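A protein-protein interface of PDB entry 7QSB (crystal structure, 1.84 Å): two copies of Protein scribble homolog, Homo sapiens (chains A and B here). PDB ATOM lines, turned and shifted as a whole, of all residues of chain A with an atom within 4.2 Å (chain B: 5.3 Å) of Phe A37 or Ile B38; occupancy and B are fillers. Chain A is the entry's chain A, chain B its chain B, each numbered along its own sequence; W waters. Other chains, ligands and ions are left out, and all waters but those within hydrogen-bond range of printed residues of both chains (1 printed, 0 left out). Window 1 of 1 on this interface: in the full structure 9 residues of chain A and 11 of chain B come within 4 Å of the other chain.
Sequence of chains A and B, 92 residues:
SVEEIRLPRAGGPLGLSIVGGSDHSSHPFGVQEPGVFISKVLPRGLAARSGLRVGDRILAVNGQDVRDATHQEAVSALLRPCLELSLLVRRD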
ATOM      1  N   ILE A  18      32.036  21.309   2.317  1.00  0.00           N
ATOM      2  CA  ILE A  18      31.354  20.067   1.969  1.00  0.00           C
ATOM      3  C   ILE A  18      30.246  19.779   2.968  1.00  0.00           C
ATOM      4  O   ILE A  18      30.314  20.182   4.133  1.00  0.00           O
ATOM      5  CB  ILE A  18      32.338  18.873   1.908  1.00  0.00           C
ATOM      6  CG1 ILE A  18      33.028  18.676   3.259  1.00  0.00           C
ATOM      7  CG2 ILE A  18      33.371  19.099   0.820  1.00  0.00           C
ATOM      8  CD1 ILE A  18      33.895  17.425   3.322  1.00  0.00           C
ATOM      9  N   VAL A  19      29.220  19.067   2.495  1.00  0.00           N
ATOM     10  CA  VAL A  19      28.119  18.588   3.322  1.00  0.00           C
ATOM     11  C   VAL A  19      28.118  17.070   3.238  1.00  0.00           C
ATOM     12  O   VAL A  19      28.034  16.506   2.140  1.00  0.00           O
ATOM     13  CB  VAL A  19      26.767  19.158   2.866  1.00  0.00           C
ATOM     14  CG1 VAL A  19      25.670  18.740   3.831  1.00  0.00           C
ATOM     15  CG2 VAL A  19      26.841  20.665   2.744  1.00  0.00           C
ATOM     16  N   GLY A  35      27.051  10.368  -2.171  1.00  0.00           N
ATOM     17  CA  GLY A  35      28.323  11.065  -2.164  1.00  0.00           C
ATOM     18  C   GLY A  35      28.343  12.214  -1.170  1.00  0.00           C
ATOM     19  O   GLY A  35      27.332  12.608  -0.594  1.00  0.00           O
ATOM     20  N   VAL A  36      29.550  12.743  -0.973  1.00  0.00           N
ATOM     21  CA  VAL A  36      29.746  13.933  -0.152  1.00  0.00           C
ATOM     22  C   VAL A  36      29.533  15.157  -1.035  1.00  0.00           C
ATOM     23  O   VAL A  36      30.237  15.341  -2.033  1.00  0.00           O
ATOM     24  CB  VAL A  36      31.140  13.949   0.494  1.00  0.00           C
ATOM     25  CG1 VAL A  36      31.357  15.258   1.236  1.00  0.00           C
ATOM     26  CG2 VAL A  36      31.295  12.759   1.436  1.00  0.00           C
ATOM     27  N   PHE A  37      28.576  16.000  -0.659  1.00  0.00           N
ATOM     28  CA  PHE A  37      28.174  17.139  -1.472  1.00  0.00           C
ATOM     29  C   PHE A  37      29.106  18.323  -1.244  1.00  0.00           C
ATOM     30  O   PHE A  37      29.350  18.729  -0.104  1.00  0.00           O
ATOM     31  CB  PHE A  37      26.721  17.503  -1.135  1.00  0.00           C
ATOM     32  CG  PHE A  37      26.199  18.689  -1.876  1.00  0.00           C
ATOM     33  CD1 PHE A  37      26.065  19.916  -1.243  1.00  0.00           C
ATOM     34  CD2 PHE A  37      25.809  18.580  -3.195  1.00  0.00           C
ATOM     35  CE1 PHE A  37      25.564  21.012  -1.924  1.00  0.00           C
ATOM     36  CE2 PHE A  37      25.312  19.672  -3.875  1.00  0.00           C
ATOM     37  CZ  PHE A  37      25.190  20.892  -3.236  1.00  0.00           C
ATOM     38  N   ILE A  38      29.644  18.863  -2.333  1.00  0.00           N
ATOM     39  CA  ILE A  38      30.476  20.055  -2.283  1.00  0.00           C
ATOM     40  C   ILE A  38      29.553  21.263  -2.372  1.00  0.00           C
ATOM     41  O   ILE A  38      28.941  21.517  -3.418  1.00  0.00           O
ATOM     42  CB  ILE A  38      31.523  20.065  -3.400  1.00  0.00           C
ATOM     43  CG1 ILE A  38      32.432  18.837  -3.273  1.00  0.00           C
ATOM     44  CG2 ILE A  38      32.348  21.350  -3.326  1.00  0.00           C
ATOM     45  CD1 ILE A  38      33.567  18.797  -4.277  1.00  0.00           C
ATOM     46  N   SER A  39      29.441  22.002  -1.272  1.00  0.00           N
ATOM     47  CA  SER A  39      28.488  23.108  -1.185  1.00  0.00           C
ATOM     48  C   SER A  39      29.073  24.435  -1.649  1.00  0.00           C
ATOM     49  O   SER A  39      28.374  25.233  -2.281  1.00  0.00           O
ATOM     50  CB  SER A  39      27.992  23.254   0.255  1.00  0.00           C
ATOM     51  OG  SER A  39      29.084  23.339   1.146  1.00  0.00           O
ATOM     52  N   GLY A  55      28.114  21.494  -6.324  1.00  0.00           N
ATOM     53  CA  GLY A  55      27.223  20.471  -6.813  1.00  0.00           C
ATOM     54  C   GLY A  55      27.868  19.116  -7.008  1.00  0.00           C
ATOM     55  O   GLY A  55      27.158  18.100  -7.055  1.00  0.00           O
ATOM     56  N   ASP A  56      29.189  19.076  -7.135  1.00  0.00           N
ATOM     57  CA  ASP A  56      29.886  17.804  -7.237  1.00  0.00           C
ATOM     58  C   ASP A  56      29.587  16.923  -6.033  1.00  0.00           C
ATOM     59  O   ASP A  56      29.278  17.406  -4.939  1.00  0.00           O
ATOM     60  CB  ASP A  56      31.403  18.044  -7.347  1.00  0.00           C
ATOM     61  CG  ASP A  56      31.816  18.568  -8.711  1.00  0.00           C
ATOM     62  OD1 ASP A  56      30.974  18.590  -9.636  1.00  0.00           O
ATOM     63  OD2 ASP A  56      32.991  18.962  -8.865  1.00  0.00           O
ATOM     64  N   ARG A  57      29.729  15.620  -6.229  1.00  0.00           N
ATOM     65  CA  ARG A  57      29.539  14.630  -5.175  1.00  0.00           C
ATOM     66  C   ARG A  57      30.792  13.765  -5.105  1.00  0.00           C
ATOM     67  O   ARG A  57      31.091  13.026  -6.045  1.00  0.00           O
ATOM     68  CB  ARG A  57      28.300  13.777  -5.450  1.00  0.00           C
ATOM     69  CG  ARG A  57      26.979  14.493  -5.232  1.00  0.00           C
ATOM     70  CD  ARG A  57      26.316  14.015  -3.949  1.00  0.00           C
ATOM     71  NE  ARG A  57      25.031  14.672  -3.703  1.00  0.00           N
ATOM     72  CZ  ARG A  57      24.345  14.561  -2.569  1.00  0.00           C
ATOM     73  NH1 ARG A  57      24.818  13.819  -1.575  1.00  0.00           N
ATOM     74  NH2 ARG A  57      23.189  15.194  -2.425  1.00  0.00           N
ATOM     75  N   LEU B  16      13.418  19.176  -7.765  1.00  0.00           N
ATOM     76  CA  LEU B  16      14.709  19.439  -7.147  1.00  0.00           C
ATOM     77  C   LEU B  16      14.976  18.388  -6.082  1.00  0.00           C
ATOM     78  O   LEU B  16      14.059  17.718  -5.598  1.00  0.00           O
ATOM     79  CB  LEU B  16      14.779  20.848  -6.524  1.00  0.00           C
ATOM     80  CG  LEU B  16      13.864  21.200  -5.357  1.00  0.00           C
ATOM     81  CD1 LEU B  16      14.193  20.448  -4.094  1.00  0.00           C
ATOM     82  CD2 LEU B  16      13.949  22.717  -5.076  1.00  0.00           C
ATOM     83  N   SER B  17      16.247  18.249  -5.720  1.00  0.00           N
ATOM     84  CA  SER B  17      16.673  17.449  -4.584  1.00  0.00           C
ATOM     85  C   SER B  17      17.427  18.349  -3.616  1.00  0.00           C
ATOM     86  O   SER B  17      18.051  19.339  -4.022  1.00  0.00           O
ATOM     87  CB  SER B  17      17.558  16.279  -5.024  1.00  0.00           C
ATOM     88  OG  SER B  17      16.901  15.510  -6.018  1.00  0.00           O
ATOM     89  N   ILE B  18      17.375  17.999  -2.331  1.00  0.00           N
ATOM     90  CA  ILE B  18      18.069  18.763  -1.301  1.00  0.00           C
ATOM     91  C   ILE B  18      18.940  17.827  -0.475  1.00  0.00           C
ATOM     92  O   ILE B  18      18.708  16.619  -0.399  1.00  0.00           O
ATOM     93  CB  ILE B  18      17.096  19.534  -0.389  1.00  0.00           C
ATOM     94  CG1 ILE B  18      16.139  18.583   0.327  1.00  0.00           C
ATOM     95  CG2 ILE B  18      16.308  20.554  -1.197  1.00  0.00           C
ATOM     96  CD1 ILE B  18      15.199  19.290   1.276  1.00  0.00           C
ATOM     97  N   VAL B  19      19.958  18.412   0.145  1.00  0.00           N
ATOM     98  CA  VAL B  19      20.933  17.685   0.946  1.00  0.00           C
ATOM     99  C   VAL B  19      21.194  18.491   2.206  1.00  0.00           C
ATOM    100  O   VAL B  19      21.050  19.717   2.217  1.00  0.00           O
ATOM    101  CB  VAL B  19      22.238  17.454   0.160  1.00  0.00           C
ATOM    102  CG1 VAL B  19      22.939  18.775  -0.093  1.00  0.00           C
ATOM    103  CG2 VAL B  19      23.144  16.484   0.906  1.00  0.00           C
ATOM    104  N   VAL B  36      20.785  23.515   4.727  1.00  0.00           N
ATOM    105  CA  VAL B  36      20.085  22.732   3.715  1.00  0.00           C
ATOM    106  C   VAL B  36      20.393  23.337   2.355  1.00  0.00           C
ATOM    107  O   VAL B  36      20.159  24.530   2.132  1.00  0.00           O
ATOM    108  CB  VAL B  36      18.569  22.702   3.976  1.00  0.00           C
ATOM    109  CG1 VAL B  36      17.823  22.160   2.771  1.00  0.00           C
ATOM    110  CG2 VAL B  36      18.274  21.870   5.221  1.00  0.00           C
ATOM    111  N   PHE B  37      20.907  22.515   1.442  1.00  0.00           N
ATOM    112  CA  PHE B  37      21.308  22.967   0.120  1.00  0.00           C
ATOM    113  C   PHE B  37      20.531  22.215  -0.954  1.00  0.00           C
ATOM    114  O   PHE B  37      20.125  21.066  -0.762  1.00  0.00           O
ATOM    115  CB  PHE B  37      22.812  22.758  -0.100  1.00  0.00           C
ATOM    116  CG  PHE B  37      23.678  23.572   0.818  1.00  0.00           C
ATOM    117  CD1 PHE B  37      23.929  23.145   2.111  1.00  0.00           C
ATOM    118  CD2 PHE B  37      24.236  24.757   0.385  1.00  0.00           C
ATOM    119  CE1 PHE B  37      24.716  23.891   2.961  1.00  0.00           C
ATOM    120  CE2 PHE B  37      25.034  25.511   1.237  1.00  0.00           C
ATOM    121  CZ  PHE B  37      25.266  25.074   2.522  1.00  0.00           C
ATOM    122  N   ILE B  38      20.353  22.871  -2.096  1.00  0.00           N
ATOM    123  CA  ILE B  38      19.778  22.232  -3.274  1.00  0.00           C
ATOM    124  C   ILE B  38      20.893  21.488  -4.000  1.00  0.00           C
ATOM    125  O   ILE B  38      21.853  22.098  -4.482  1.00  0.00           O
ATOM    126  CB  ILE B  38      19.102  23.263  -4.189  1.00  0.00           C
ATOM    127  CG1 ILE B  38      18.036  24.029  -3.395  1.00  0.00           C
ATOM    128  CG2 ILE B  38      18.493  22.583  -5.392  1.00  0.00           C
ATOM    129  CD1 ILE B  38      17.220  25.008  -4.224  1.00  0.00           C
ATOM    130  N   SER B  39      20.767  20.166  -4.077  1.00  0.00           N
ATOM    131  CA  SER B  39      21.810  19.334  -4.672  1.00  0.00           C
ATOM    132  C   SER B  39      21.582  19.054  -6.149  1.00  0.00           C
ATOM    133  O   SER B  39      22.554  18.923  -6.901  1.00  0.00           O
ATOM    134  CB  SER B  39      21.917  18.006  -3.919  1.00  0.00           C
ATOM    135  OG  SER B  39      20.661  17.351  -3.881  1.00  0.00           O
ATOM    136  N   LYS B  40      20.330  18.962  -6.587  1.00  0.00           N
ATOM    137  CA  LYS B  40      20.028  18.726  -7.989  1.00  0.00           C
ATOM    138  C   LYS B  40      18.807  19.539  -8.387  1.00  0.00           C
ATOM    139  O   LYS B  40      17.886  19.737  -7.589  1.00  0.00           O
ATOM    140  CB  LYS B  40      19.767  17.238  -8.283  1.00  0.00           C
ATOM    141  CG  LYS B  40      20.955  16.329  -8.018  1.00  0.00           C
ATOM    142  CD  LYS B  40      20.711  14.928  -8.574  1.00  0.00           C
ATOM    143  CE  LYS B  40      21.098  14.843 -10.043  1.00  0.00           C
ATOM    144  NZ  LYS B  40      20.557  13.611 -10.701  1.00  0.00           N
ATOM    145  N   VAL B  41      18.811  19.999  -9.637  1.00  0.00           N
ATOM    146  CA  VAL B  41      17.709  20.762 -10.215  1.00  0.00           C
ATOM    147  C   VAL B  41      17.437  20.197 -11.603  1.00  0.00           C
ATOM    148  O   VAL B  41      18.319  20.225 -12.468  1.00  0.00           O
ATOM    149  CB  VAL B  41      18.035  22.265 -10.297  1.00  0.00           C
ATOM    150  CG1 VAL B  41      17.017  22.989 -11.147  1.00  0.00           C
ATOM    151  CG2 VAL B  41      18.077  22.855  -8.893  1.00  0.00           C
ATOM    152  N   LEU B  52      15.642  28.568  -8.947  1.00  0.00           N
ATOM    153  CA  LEU B  52      16.484  27.844  -8.004  1.00  0.00           C
ATOM    154  C   LEU B  52      17.645  27.181  -8.737  1.00  0.00           C
ATOM    155  O   LEU B  52      17.525  26.751  -9.887  1.00  0.00           O
ATOM    156  CB  LEU B  52      15.660  26.798  -7.254  1.00  0.00           C
ATOM    157  CG  LEU B  52      14.558  27.354  -6.355  1.00  0.00           C
ATOM    158  CD1 LEU B  52      13.629  26.243  -5.883  1.00  0.00           C
ATOM    159  CD2 LEU B  52      15.157  28.096  -5.150  1.00  0.00           C
ATOM    160  N   ARG B  53      18.797  27.118  -8.062  1.00  0.00           N
ATOM    161  CA  ARG B  53      20.008  26.591  -8.662  1.00  0.00           C
ATOM    162  C   ARG B  53      20.687  25.616  -7.713  1.00  0.00           C
ATOM    163  O   ARG B  53      20.551  25.714  -6.489  1.00  0.00           O
ATOM    164  CB  ARG B  53      20.997  27.711  -9.011  1.00  0.00           C
ATOM    165  CG  ARG B  53      20.435  28.846  -9.842  1.00  0.00           C
ATOM    166  CD  ARG B  53      21.544  29.868 -10.112  1.00  0.00           C
ATOM    167  NE  ARG B  53      21.036  31.168 -10.541  1.00  0.00           N
ATOM    168  CZ  ARG B  53      21.786  32.266 -10.636  1.00  0.00           C
ATOM    169  NH1 ARG B  53      21.243  33.409 -11.029  1.00  0.00           N
ATOM    170  NH2 ARG B  53      23.078  32.219 -10.332  1.00  0.00           N
ATOM    171  N   VAL B  54      21.432  24.674  -8.297  1.00  0.00           N
ATOM    172  CA  VAL B  54      22.281  23.801  -7.501  1.00  0.00           C
ATOM    173  C   VAL B  54      23.231  24.652  -6.668  1.00  0.00           C
ATOM    174  O   VAL B  54      23.817  25.623  -7.157  1.00  0.00           O
ATOM    175  CB  VAL B  54      23.056  22.835  -8.410  1.00  0.00           C
ATOM    176  CG1 VAL B  54      24.123  22.091  -7.609  1.00  0.00           C
ATOM    177  CG2 VAL B  54      22.102  21.863  -9.088  1.00  0.00           C
ATOM    178  N   GLY B  55      23.394  24.279  -5.403  1.00  0.00           N
ATOM    179  CA  GLY B  55      24.251  24.996  -4.489  1.00  0.00           C
ATOM    180  C   GLY B  55      23.564  26.042  -3.641  1.00  0.00           C
ATOM    181  O   GLY B  55      24.138  26.481  -2.633  1.00  0.00           O
ATOM    182  N   ASP B  56      22.357  26.460  -4.020  1.00  0.00           N
ATOM    183  CA  ASP B  56      21.611  27.404  -3.203  1.00  0.00           C
ATOM    184  C   ASP B  56      21.392  26.831  -1.809  1.00  0.00           C
ATOM    185  O   ASP B  56      21.066  25.650  -1.649  1.00  0.00           O
ATOM    186  CB  ASP B  56      20.258  27.718  -3.854  1.00  0.00           C
ATOM    187  CG  ASP B  56      20.392  28.528  -5.124  1.00  0.00           C
ATOM    188  OD1 ASP B  56      21.521  28.923  -5.470  1.00  0.00           O
ATOM    189  OD2 ASP B  56      19.357  28.778  -5.777  1.00  0.00           O
ATOM    190  N   ARG B  57      21.560  27.676  -0.797  1.00  0.00           N
ATOM    191  CA  ARG B  57      21.245  27.316   0.578  1.00  0.00           C
ATOM    192  C   ARG B  57      19.856  27.848   0.905  1.00  0.00           C
ATOM    193  O   ARG B  57      19.594  29.043   0.745  1.00  0.00           O
ATOM    194  CB  ARG B  57      22.270  27.883   1.565  1.00  0.00           C
ATOM    195  CG  ARG B  57      21.945  27.522   3.005  1.00  0.00           C
ATOM    196  CD  ARG B  57      22.986  28.006   4.000  1.00  0.00           C
ATOM    197  NE  ARG B  57      22.631  27.585   5.354  1.00  0.00           N
ATOM    198  CZ  ARG B  57      23.461  27.599   6.392  1.00  0.00           C
ATOM    199  NH1 ARG B  57      24.711  28.011   6.242  1.00  0.00           N
ATOM    200  NH2 ARG B  57      23.038  27.189   7.580  1.00  0.00           N
ATOM    201  N   ILE B  58      18.970  26.964   1.351  1.00  0.00           N
ATOM    202  CA  ILE B  58      17.608  27.350   1.696  1.00  0.00           C
ATOM    203  C   ILE B  58      17.632  27.933   3.105  1.00  0.00           C
ATOM    204  O   ILE B  58      17.876  27.219   4.080  1.00  0.00           O
ATOM    205  CB  ILE B  58      16.644  26.164   1.597  1.00  0.00           C
ATOM    206  CG1 ILE B  58      16.718  25.549   0.194  1.00  0.00           C
ATOM    207  CG2 ILE B  58      15.240  26.609   1.919  1.00  0.00           C
ATOM    208  CD1 ILE B  58      15.887  24.287   0.025  1.00  0.00           C
ATOM    209  N   VAL B  89      16.791  32.031  -0.409  1.00  0.00           N
ATOM    210  CA  VAL B  89      18.018  31.273  -0.618  1.00  0.00           C
ATOM    211  C   VAL B  89      19.234  32.190  -0.651  1.00  0.00           C
ATOM    212  O   VAL B  89      19.135  33.366  -1.015  1.00  0.00           O
ATOM    213  CB  VAL B  89      17.954  30.432  -1.917  1.00  0.00           C
ATOM    214  CG1 VAL B  89      16.773  29.477  -1.856  1.00  0.00           C
ATOM    215  CG2 VAL B  89      17.874  31.318  -3.145  1.00  0.00           C
HETATM  216  O   HOH W   1      26.626  27.335  -2.769  1.00  0.00           O
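O of Ile B38 lies within hydrogen-bond range of N of Gly B55.
The backbone carbonyl oxygen (O) of Asp B56 is in hydrogen-bond range of the backbone NH (N) of Ile B38 (2.9 Å).
The backbone carbonyl oxygen (O) of Gly A35 is in hydrogen-bond range of the guanidinium group (NH1) of Arg A57, at 3.0 Å.
The backbone NH (N) of Ser B39 is in hydrogen-bond range of the backbone carbonyl oxygen (O) of Ser B17 (2.8 Å).
The backbone NH (N) of Val A19 sits at hydrogen-bond distance from the backbone carbonyl oxygen (O) of Phe A37.
O of Ile A38 lies within hydrogen-bond range of N of Gly A55 (3.0 Å).
Val A19 touches Phe B37, and with the chains exchanged Phe A37 touches Val B19.
Phe A37 touches Ile B38, but with the chains exchanged Ile A38 does not touch Phe B37 (6.9 Å).
Phe A37 touches Ser B39, and with the chains exchanged Ser A39 touches Phe B37.
Arg A57 touches Val B19, but with the chains exchanged Val A19 does not touch Arg B57 (8.4 Å).
Of the 9 pairs that touch across the chains among the printed residues, 5 have their exchanged pair printed and touching as well.
Phe B37 touches Val A19.
CD1 of Phe A37 touches CG1 of Val B19, 3.5 Å away.
Phe A37 touches Phe B37.
O of Ile B38 touches CZ of Phe A37 (3.8 Å).
Ser B39 touches Phe A37.
Ser A39 touches Phe B37.
CA of Gly A55 touches CG1 of Val B54, at 3.6 Å.
NH2 of Arg A57 touches CB of Val B19 (3.6 Å).
Arg A57 touches Ser B39.
Hydrophobic or aromatic side chains of chain B that line the printed part of chain A: Val B19, Phe B37 and Val B54.
Among the printed residues, no Asp or Glu carboxylate lies within 4 Å of a Lys or Arg side-chain nitrogen of the other chain.
Of chain B, only Val B19 (3.5 Å), Phe B37 (3.7 Å), Ile B38 (3.8 Å) and Ser B39 (3.6 Å) come within 4 Å of Phe A37.
Of the printed residues of chain B, Ser A39 touches Phe B37 (3.8 Å).
Of the printed residues of chain B, Arg A57 touches Val B19 (3.6 Å) and Ser B39 (3.4 Å).
Printed residues of chain A within 4 Å of Val B19: Phe A37 and Arg A57.
Printed residues of chain A within 4 Å of Ile B38: Phe A37 (3.8 Å).
Val B41 touches none of the printed residues of chain A.
The nearest printed residue of chain B that does not touch Val A19 is Val B19 (4.5 Å).
Water W1 lies within hydrogen-bond range of the backbone carbonyl oxygen (O) of Gly B55 (2.6 Å) and the backbone carbonyl oxygen (O) of Ser A39 (2.8 Å).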
